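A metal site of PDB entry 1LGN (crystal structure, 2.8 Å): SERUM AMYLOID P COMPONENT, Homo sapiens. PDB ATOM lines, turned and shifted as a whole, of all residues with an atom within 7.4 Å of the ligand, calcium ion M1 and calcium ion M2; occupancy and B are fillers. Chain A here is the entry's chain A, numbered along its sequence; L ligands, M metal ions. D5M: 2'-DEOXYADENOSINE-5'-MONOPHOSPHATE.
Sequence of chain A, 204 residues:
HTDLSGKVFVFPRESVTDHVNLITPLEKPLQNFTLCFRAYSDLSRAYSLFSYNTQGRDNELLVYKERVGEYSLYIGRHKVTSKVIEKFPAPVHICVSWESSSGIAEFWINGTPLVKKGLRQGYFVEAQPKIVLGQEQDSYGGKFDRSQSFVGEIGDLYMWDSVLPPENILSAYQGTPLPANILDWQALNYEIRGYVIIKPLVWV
A nitrogen (N6) of the ligand lies within hydrogen-bond range of the side-chain hydroxyl of Ser 147. An oxygen (O4') of the ligand lies within hydrogen-bond range of the side-chain hydroxyl (OH) of Tyr 64. OD1 of Asp 145 is in hydrogen-bond range of N6 of the ligand (3.2 Å). The side-chain hydroxyl (OH) of Tyr 74 lies within hydrogen-bond range of an oxygen (O3') of the ligand, at 3.4 Å.
The backbone NH (N) of Asn 59 sits at hydrogen-bond distance from the side-chain amide oxygen (OD1) of Asn 53 (3.1 Å). The backbone NH (N) of Asp 138 lies close to the backbone carbonyl oxygen (O) of Lys 143, at 3.4 Å. OH of Tyr 64 sits at hydrogen-bond distance from NE2 of Gln 148, 2.7 Å away. The backbone NH (N) of Gln 137 is in hydrogen-bond range of the side-chain hydroxyl (OG) of Ser 51 (3.3 Å). The side-chain amide oxygen (OE1) of Gln 137 lies close to the backbone carbonyl oxygen (O) of Ser 139 (3.4 Å). OG of Ser 147 is in hydrogen-bond range of OD1 of Asp 145, 2.7 Å away. NZ of Lys 79 sits close to OH of Tyr 74, 3.5 Å away. The backbone NH (N) of Tyr 74 sits at hydrogen-bond distance from the backbone carbonyl oxygen (O) of Leu 62 (2.9 Å).
Hydrophobic or aromatic side chains within 4 Å of the ligand: Tyr 64. Within 4 Å of the ligand: Asp 58, Asn 59, Tyr 64, Tyr 74, Glu 136, Asp 138, Asp 145, Ser 147 and Gln 148. The nearest printed residue that does not touch the ligand is Lys 79 (4.3 Å).
Residues that only touch calcium ion M1: Asp 145 (3.8 Å). Within 4 Å of calcium ion M1: Glu 136, Asp 138, Asp 145 and Gln 148. The nearest printed residue that does not touch calcium ion M1 is Gln 137 (4.7 Å).
The nearest printed residue that does not touch calcium ion M2 is Asn 53 (5.0 Å).
The side-chain carboxylate (OD2) of Asp 138 binds calcium ion M1 (2.4 Å). O3P of the ligand is bound to calcium ion M1, at 2.4 Å. Calcium ion M1 is bound by OE1 of Glu 136, 2.4 Å away. Calcium ion M1 is bound by OE1 of Gln 148 (2.4 Å). The side-chain carboxylate (OD1) of Asp 138 is bound to calcium ion M1 (2.7 Å).
Calcium ion M2 is bound by O2P of the ligand (2.3 Å), OE2 of Glu 136 (2.3 Å), OD1 of Asn 59 (2.3 Å), OD1 of Asp 138 (2.4 Å), OD1 of Asp 58 (2.5 Å), O of Gln 137 (2.5 Å), OE1 of Glu 136 (2.9 Å) and OD2 of Asp 58 (2.9 Å).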
ATOM      1  N   ALA A  46      -7.183  12.849  -2.438  1.00  0.00           N
ATOM      2  CA  ALA A  46      -7.685  14.179  -2.736  1.00  0.00           C
ATOM      3  C   ALA A  46      -7.148  14.552  -4.092  1.00  0.00           C
ATOM      4  O   ALA A  46      -6.103  14.056  -4.526  1.00  0.00           O
ATOM      5  CB  ALA A  46      -7.211  15.162  -1.708  1.00  0.00           C
ATOM      6  N   SER A  51      -8.484  24.300 -11.285  1.00  0.00           N
ATOM      7  CA  SER A  51      -7.507  25.242 -10.737  1.00  0.00           C
ATOM      8  C   SER A  51      -7.513  26.553 -11.512  1.00  0.00           C
ATOM      9  O   SER A  51      -7.553  26.552 -12.733  1.00  0.00           O
ATOM     10  CB  SER A  51      -6.107  24.613 -10.756  1.00  0.00           C
ATOM     11  OG  SER A  51      -5.195  25.327  -9.934  1.00  0.00           O
ATOM     12  N   ASN A  53      -5.383  30.246 -11.148  1.00  0.00           N
ATOM     13  CA  ASN A  53      -4.392  31.098 -10.508  1.00  0.00           C
ATOM     14  C   ASN A  53      -4.105  32.331 -11.348  1.00  0.00           C
ATOM     15  O   ASN A  53      -4.191  32.287 -12.570  1.00  0.00           O
ATOM     16  CB  ASN A  53      -3.059  30.366 -10.337  1.00  0.00           C
ATOM     17  CG  ASN A  53      -3.043  29.476  -9.140  1.00  0.00           C
ATOM     18  OD1 ASN A  53      -4.082  29.083  -8.618  1.00  0.00           O
ATOM     19  ND2 ASN A  53      -1.831  29.146  -8.686  1.00  0.00           N
ATOM     20  N   ASP A  58      -1.763  32.298  -5.413  1.00  0.00           N
ATOM     21  CA  ASP A  58      -2.032  30.872  -5.495  1.00  0.00           C
ATOM     22  C   ASP A  58      -3.451  30.600  -4.988  1.00  0.00           C
ATOM     23  O   ASP A  58      -3.927  31.274  -4.099  1.00  0.00           O
ATOM     24  CB  ASP A  58      -1.019  30.103  -4.645  1.00  0.00           C
ATOM     25  CG  ASP A  58      -1.170  28.583  -4.737  1.00  0.00           C
ATOM     26  OD1 ASP A  58      -1.687  28.071  -5.753  1.00  0.00           O
ATOM     27  OD2 ASP A  58      -0.752  27.876  -3.803  1.00  0.00           O
ATOM     28  N   ASN A  59      -4.110  29.608  -5.567  1.00  0.00           N
ATOM     29  CA  ASN A  59      -5.472  29.258  -5.177  1.00  0.00           C
ATOM     30  C   ASN A  59      -6.347  30.503  -5.167  1.00  0.00           C
ATOM     31  O   ASN A  59      -6.877  30.891  -4.135  1.00  0.00           O
ATOM     32  CB  ASN A  59      -5.493  28.604  -3.797  1.00  0.00           C
ATOM     33  CG  ASN A  59      -4.535  27.427  -3.671  1.00  0.00           C
ATOM     34  OD1 ASN A  59      -4.172  26.785  -4.662  1.00  0.00           O
ATOM     35  ND2 ASN A  59      -4.097  27.153  -2.453  1.00  0.00           N
ATOM     36  N   GLU A  60      -6.444  31.171  -6.316  1.00  0.00           N
ATOM     37  CA  GLU A  60      -7.277  32.356  -6.400  1.00  0.00           C
ATOM     38  C   GLU A  60      -8.715  31.870  -6.484  1.00  0.00           C
ATOM     39  O   GLU A  60      -9.610  32.468  -5.913  1.00  0.00           O
ATOM     40  CB  GLU A  60      -6.886  33.213  -7.604  1.00  0.00           C
ATOM     41  CG  GLU A  60      -7.653  34.523  -7.717  1.00  0.00           C
ATOM     42  CD  GLU A  60      -7.386  35.482  -6.569  1.00  0.00           C
ATOM     43  OE1 GLU A  60      -6.459  35.243  -5.783  1.00  0.00           O
ATOM     44  OE2 GLU A  60      -8.107  36.483  -6.464  1.00  0.00           O
ATOM     45  N   LEU A  62     -10.159  27.798  -6.620  1.00  0.00           N
ATOM     46  CA  LEU A  62      -9.867  26.348  -6.695  1.00  0.00           C
ATOM     47  C   LEU A  62     -11.013  25.491  -6.170  1.00  0.00           C
ATOM     48  O   LEU A  62     -11.506  25.727  -5.076  1.00  0.00           O
ATOM     49  CB  LEU A  62      -8.602  26.044  -5.874  1.00  0.00           C
ATOM     50  CG  LEU A  62      -8.252  24.636  -5.414  1.00  0.00           C
ATOM     51  CD1 LEU A  62      -8.021  23.760  -6.583  1.00  0.00           C
ATOM     52  CD2 LEU A  62      -6.992  24.664  -4.550  1.00  0.00           C
ATOM     53  N   TYR A  64     -11.539  22.023  -4.977  1.00  0.00           N
ATOM     54  CA  TYR A  64     -10.753  20.877  -4.542  1.00  0.00           C
ATOM     55  C   TYR A  64     -11.584  19.816  -3.849  1.00  0.00           C
ATOM     56  O   TYR A  64     -12.497  20.160  -3.106  1.00  0.00           O
ATOM     57  CB  TYR A  64      -9.710  21.389  -3.568  1.00  0.00           C
ATOM     58  CG  TYR A  64      -8.560  20.488  -3.273  1.00  0.00           C
ATOM     59  CD1 TYR A  64      -7.555  20.256  -4.214  1.00  0.00           C
ATOM     60  CD2 TYR A  64      -8.406  19.946  -2.015  1.00  0.00           C
ATOM     61  CE1 TYR A  64      -6.424  19.508  -3.900  1.00  0.00           C
ATOM     62  CE2 TYR A  64      -7.287  19.193  -1.697  1.00  0.00           C
ATOM     63  CZ  TYR A  64      -6.300  18.986  -2.638  1.00  0.00           C
ATOM     64  OH  TYR A  64      -5.185  18.285  -2.289  1.00  0.00           O
ATOM     65  N   GLU A  66     -11.523  17.042  -1.099  1.00  0.00           N
ATOM     66  CA  GLU A  66     -10.828  16.532   0.080  1.00  0.00           C
ATOM     67  C   GLU A  66     -10.821  15.018   0.239  1.00  0.00           C
ATOM     68  O   GLU A  66      -9.799  14.414   0.553  1.00  0.00           O
ATOM     69  CB  GLU A  66     -11.498  17.127   1.313  1.00  0.00           C
ATOM     70  CG  GLU A  66     -11.502  18.643   1.324  1.00  0.00           C
ATOM     71  CD  GLU A  66     -10.107  19.221   1.447  1.00  0.00           C
ATOM     72  OE1 GLU A  66      -9.188  18.495   1.920  1.00  0.00           O
ATOM     73  OE2 GLU A  66      -9.924  20.407   1.084  1.00  0.00           O
ATOM     74  N   TYR A  74     -11.955  27.401  -2.704  1.00  0.00           N
ATOM     75  CA  TYR A  74     -11.002  28.405  -2.265  1.00  0.00           C
ATOM     76  C   TYR A  74     -11.260  29.691  -3.050  1.00  0.00           C
ATOM     77  O   TYR A  74     -11.486  29.644  -4.261  1.00  0.00           O
ATOM     78  CB  TYR A  74      -9.589  27.966  -2.571  1.00  0.00           C
ATOM     79  CG  TYR A  74      -8.998  26.913  -1.682  1.00  0.00           C
ATOM     80  CD1 TYR A  74      -9.434  25.582  -1.731  1.00  0.00           C
ATOM     81  CD2 TYR A  74      -7.938  27.224  -0.812  1.00  0.00           C
ATOM     82  CE1 TYR A  74      -8.825  24.585  -0.954  1.00  0.00           C
ATOM     83  CE2 TYR A  74      -7.330  26.234  -0.027  1.00  0.00           C
ATOM     84  CZ  TYR A  74      -7.776  24.925  -0.104  1.00  0.00           C
ATOM     85  OH  TYR A  74      -7.184  23.944   0.668  1.00  0.00           O
ATOM     86  N   LYS A  79     -10.802  29.286   2.331  1.00  0.00           N
ATOM     87  CA  LYS A  79     -11.483  28.046   2.012  1.00  0.00           C
ATOM     88  C   LYS A  79     -12.746  27.695   2.777  1.00  0.00           C
ATOM     89  O   LYS A  79     -12.878  28.009   3.958  1.00  0.00           O
ATOM     90  CB  LYS A  79     -10.449  26.956   2.233  1.00  0.00           C
ATOM     91  CG  LYS A  79     -10.924  25.549   2.253  1.00  0.00           C
ATOM     92  CD  LYS A  79      -9.817  24.689   2.820  1.00  0.00           C
ATOM     93  CE  LYS A  79     -10.074  23.223   2.539  1.00  0.00           C
ATOM     94  NZ  LYS A  79      -9.037  22.360   3.161  1.00  0.00           N
ATOM     95  N   GLN A 135      -4.530  19.160 -13.011  1.00  0.00           N
ATOM     96  CA  GLN A 135      -3.402  19.385 -12.120  1.00  0.00           C
ATOM     97  C   GLN A 135      -3.745  20.529 -11.176  1.00  0.00           C
ATOM     98  O   GLN A 135      -4.749  21.223 -11.375  1.00  0.00           O
ATOM     99  CB  GLN A 135      -2.161  19.766 -12.909  1.00  0.00           C
ATOM    100  CG  GLN A 135      -1.594  18.663 -13.742  1.00  0.00           C
ATOM    101  CD  GLN A 135      -1.113  17.513 -12.913  1.00  0.00           C
ATOM    102  OE1 GLN A 135      -0.839  17.667 -11.713  1.00  0.00           O
ATOM    103  NE2 GLN A 135      -1.023  16.355 -13.536  1.00  0.00           N
ATOM    104  N   GLU A 136      -2.952  20.699 -10.133  1.00  0.00           N
ATOM    105  CA  GLU A 136      -3.206  21.781  -9.194  1.00  0.00           C
ATOM    106  C   GLU A 136      -1.998  22.691  -9.228  1.00  0.00           C
ATOM    107  O   GLU A 136      -0.866  22.287  -8.886  1.00  0.00           O
ATOM    108  CB  GLU A 136      -3.476  21.225  -7.783  1.00  0.00           C
ATOM    109  CG  GLU A 136      -4.199  22.184  -6.834  1.00  0.00           C
ATOM    110  CD  GLU A 136      -3.291  23.265  -6.245  1.00  0.00           C
ATOM    111  OE1 GLU A 136      -2.178  22.943  -5.768  1.00  0.00           O
ATOM    112  OE2 GLU A 136      -3.698  24.448  -6.244  1.00  0.00           O
ATOM    113  N   GLN A 137      -2.234  23.905  -9.691  1.00  0.00           N
ATOM    114  CA  GLN A 137      -1.160  24.885  -9.813  1.00  0.00           C
ATOM    115  C   GLN A 137      -0.728  25.412  -8.468  1.00  0.00           C
ATOM    116  O   GLN A 137      -1.548  25.588  -7.573  1.00  0.00           O
ATOM    117  CB  GLN A 137      -1.618  26.082 -10.632  1.00  0.00           C
ATOM    118  CG  GLN A 137      -1.986  25.815 -12.055  1.00  0.00           C
ATOM    119  CD  GLN A 137      -2.743  26.984 -12.654  1.00  0.00           C
ATOM    120  OE1 GLN A 137      -2.167  28.054 -12.866  1.00  0.00           O
ATOM    121  NE2 GLN A 137      -4.040  26.799 -12.917  1.00  0.00           N
ATOM    122  N   ASP A 138       0.560  25.648  -8.330  1.00  0.00           N
ATOM    123  CA  ASP A 138       1.115  26.244  -7.127  1.00  0.00           C
ATOM    124  C   ASP A 138       1.901  27.467  -7.566  1.00  0.00           C
ATOM    125  O   ASP A 138       2.566  28.126  -6.780  1.00  0.00           O
ATOM    126  CB  ASP A 138       1.988  25.276  -6.343  1.00  0.00           C
ATOM    127  CG  ASP A 138       1.183  24.372  -5.429  1.00  0.00           C
ATOM    128  OD1 ASP A 138      -0.032  24.635  -5.258  1.00  0.00           O
ATOM    129  OD2 ASP A 138       1.779  23.408  -4.879  1.00  0.00           O
ATOM    130  N   SER A 139       1.791  27.765  -8.856  1.00  0.00           N
ATOM    131  CA  SER A 139       2.425  28.906  -9.486  1.00  0.00           C
ATOM    132  C   SER A 139       1.501  29.311 -10.640  1.00  0.00           C
ATOM    133  O   SER A 139       0.453  28.696 -10.853  1.00  0.00           O
ATOM    134  CB  SER A 139       3.822  28.545  -9.994  1.00  0.00           C
ATOM    135  OG  SER A 139       3.773  27.673 -11.103  1.00  0.00           O
ATOM    136  N   GLY A 142       1.854  26.668 -13.358  1.00  0.00           N
ATOM    137  CA  GLY A 142       2.767  25.574 -13.120  1.00  0.00           C
ATOM    138  C   GLY A 142       2.884  25.024 -11.703  1.00  0.00           C
ATOM    139  O   GLY A 142       1.945  25.097 -10.906  1.00  0.00           O
ATOM    140  N   LYS A 143       4.055  24.462 -11.416  1.00  0.00           N
ATOM    141  CA  LYS A 143       4.383  23.835 -10.139  1.00  0.00           C
ATOM    142  C   LYS A 143       3.305  22.851  -9.686  1.00  0.00           C
ATOM    143  O   LYS A 143       2.681  23.016  -8.638  1.00  0.00           O
ATOM    144  CB  LYS A 143       4.693  24.878  -9.067  1.00  0.00           C
ATOM    145  N   PHE A 144       3.117  21.813 -10.495  1.00  0.00           N
ATOM    146  CA  PHE A 144       2.138  20.762 -10.258  1.00  0.00           C
ATOM    147  C   PHE A 144       2.581  19.750  -9.209  1.00  0.00           C
ATOM    148  O   PHE A 144       3.766  19.405  -9.130  1.00  0.00           O
ATOM    149  CB  PHE A 144       1.841  20.041 -11.569  1.00  0.00           C
ATOM    150  CG  PHE A 144       1.283  20.932 -12.633  1.00  0.00           C
ATOM    151  CD1 PHE A 144       0.643  22.119 -12.301  1.00  0.00           C
ATOM    152  CD2 PHE A 144       1.393  20.584 -13.965  1.00  0.00           C
ATOM    153  CE1 PHE A 144       0.114  22.931 -13.283  1.00  0.00           C
ATOM    154  CE2 PHE A 144       0.864  21.396 -14.947  1.00  0.00           C
ATOM    155  CZ  PHE A 144       0.222  22.570 -14.614  1.00  0.00           C
ATOM    156  N   ASP A 145       1.610  19.299  -8.404  1.00  0.00           N
ATOM    157  CA  ASP A 145       1.855  18.283  -7.396  1.00  0.00           C
ATOM    158  C   ASP A 145       0.998  17.046  -7.684  1.00  0.00           C
ATOM    159  O   ASP A 145      -0.248  17.143  -7.618  1.00  0.00           O
ATOM    160  CB  ASP A 145       1.642  18.841  -5.986  1.00  0.00           C
ATOM    161  CG  ASP A 145       2.430  18.054  -4.948  1.00  0.00           C
ATOM    162  OD1 ASP A 145       2.192  16.827  -4.840  1.00  0.00           O
ATOM    163  OD2 ASP A 145       3.269  18.651  -4.246  1.00  0.00           O
ATOM    164  N   ARG A 146       1.774  15.991  -7.997  1.00  0.00           N
ATOM    165  CA  ARG A 146       1.332  14.657  -8.417  1.00  0.00           C
ATOM    166  C   ARG A 146       0.281  14.077  -7.535  1.00  0.00           C
ATOM    167  O   ARG A 146      -0.637  13.416  -8.031  1.00  0.00           O
ATOM    168  CB  ARG A 146       2.510  13.648  -8.472  1.00  0.00           C
ATOM    169  CG  ARG A 146       2.056  12.221  -8.784  1.00  0.00           C
ATOM    170  CD  ARG A 146       3.167  11.194  -8.547  1.00  0.00           C
ATOM    171  NE  ARG A 146       3.810  10.788  -9.789  1.00  0.00           N
ATOM    172  CZ  ARG A 146       3.353   9.842 -10.609  1.00  0.00           C
ATOM    173  NH1 ARG A 146       2.232   9.190 -10.338  1.00  0.00           N
ATOM    174  NH2 ARG A 146       4.034   9.544 -11.725  1.00  0.00           N
ATOM    175  N   SER A 147       0.414  14.304  -6.256  1.00  0.00           N
ATOM    176  CA  SER A 147      -0.534  13.778  -5.312  1.00  0.00           C
ATOM    177  C   SER A 147      -1.857  14.546  -5.320  1.00  0.00           C
ATOM    178  O   SER A 147      -2.760  14.248  -4.547  1.00  0.00           O
ATOM    179  CB  SER A 147       0.054  13.752  -3.896  1.00  0.00           C
ATOM    180  OG  SER A 147       0.695  14.983  -3.588  1.00  0.00           O
ATOM    181  N   GLN A 148      -1.956  15.535  -6.196  1.00  0.00           N
ATOM    182  CA  GLN A 148      -3.180  16.312  -6.325  1.00  0.00           C
ATOM    183  C   GLN A 148      -3.736  16.199  -7.727  1.00  0.00           C
ATOM    184  O   GLN A 148      -4.797  16.740  -8.002  1.00  0.00           O
ATOM    185  CB  GLN A 148      -2.942  17.784  -5.975  1.00  0.00           C
ATOM    186  CG  GLN A 148      -2.612  17.972  -4.526  1.00  0.00           C
ATOM    187  CD  GLN A 148      -2.426  19.409  -4.159  1.00  0.00           C
ATOM    188  OE1 GLN A 148      -1.669  20.132  -4.805  1.00  0.00           O
ATOM    189  NE2 GLN A 148      -3.089  19.830  -3.093  1.00  0.00           N
HETATM  190  O5' D5M L   1      -2.870  23.404  -1.092  1.00  0.00           O
HETATM  191  C5' D5M L   1      -4.143  22.885  -1.392  1.00  0.00           C
HETATM  192  C4' D5M L   1      -4.499  21.867  -0.304  1.00  0.00           C
HETATM  193  O4' D5M L   1      -3.878  20.593  -0.567  1.00  0.00           O
HETATM  194  C3' D5M L   1      -3.973  22.310   1.046  1.00  0.00           C
HETATM  195  O3' D5M L   1      -4.871  21.851   2.027  1.00  0.00           O
HETATM  196  C2' D5M L   1      -2.696  21.544   1.247  1.00  0.00           C
HETATM  197  C1' D5M L   1      -2.955  20.275   0.483  1.00  0.00           C
HETATM  198  N9  D5M L   1      -1.737  19.823  -0.165  1.00  0.00           N
HETATM  199  C8  D5M L   1      -0.848  20.510  -0.918  1.00  0.00           C
HETATM  200  N7  D5M L   1       0.150  19.818  -1.377  1.00  0.00           N
HETATM  201  C5  D5M L   1      -0.088  18.561  -0.890  1.00  0.00           C
HETATM  202  C6  D5M L   1       0.604  17.341  -1.020  1.00  0.00           C
HETATM  203  N6  D5M L   1       1.719  17.193  -1.731  1.00  0.00           N
HETATM  204  N1  D5M L   1       0.099  16.248  -0.380  1.00  0.00           N
HETATM  205  C2  D5M L   1      -1.025  16.398   0.328  1.00  0.00           C
HETATM  206  N3  D5M L   1      -1.785  17.507   0.500  1.00  0.00           N
HETATM  207  C4  D5M L   1      -1.243  18.552  -0.140  1.00  0.00           C
HETATM  208  P   D5M L   1      -1.807  23.843  -2.180  1.00  0.00           P
HETATM  209  O1P D5M L   1      -0.660  24.333  -1.352  1.00  0.00           O
HETATM  210  O3P D5M L   1      -1.385  22.658  -3.017  1.00  0.00           O
HETATM  211  O2P D5M L   1      -2.498  24.920  -3.003  1.00  0.00           O
HETATM  212 CA    CA M   1      -0.111  21.998  -4.935  1.00  0.00          CA
HETATM  213 CA    CA M   2      -2.131  25.720  -5.109  1.00  0.00          CA
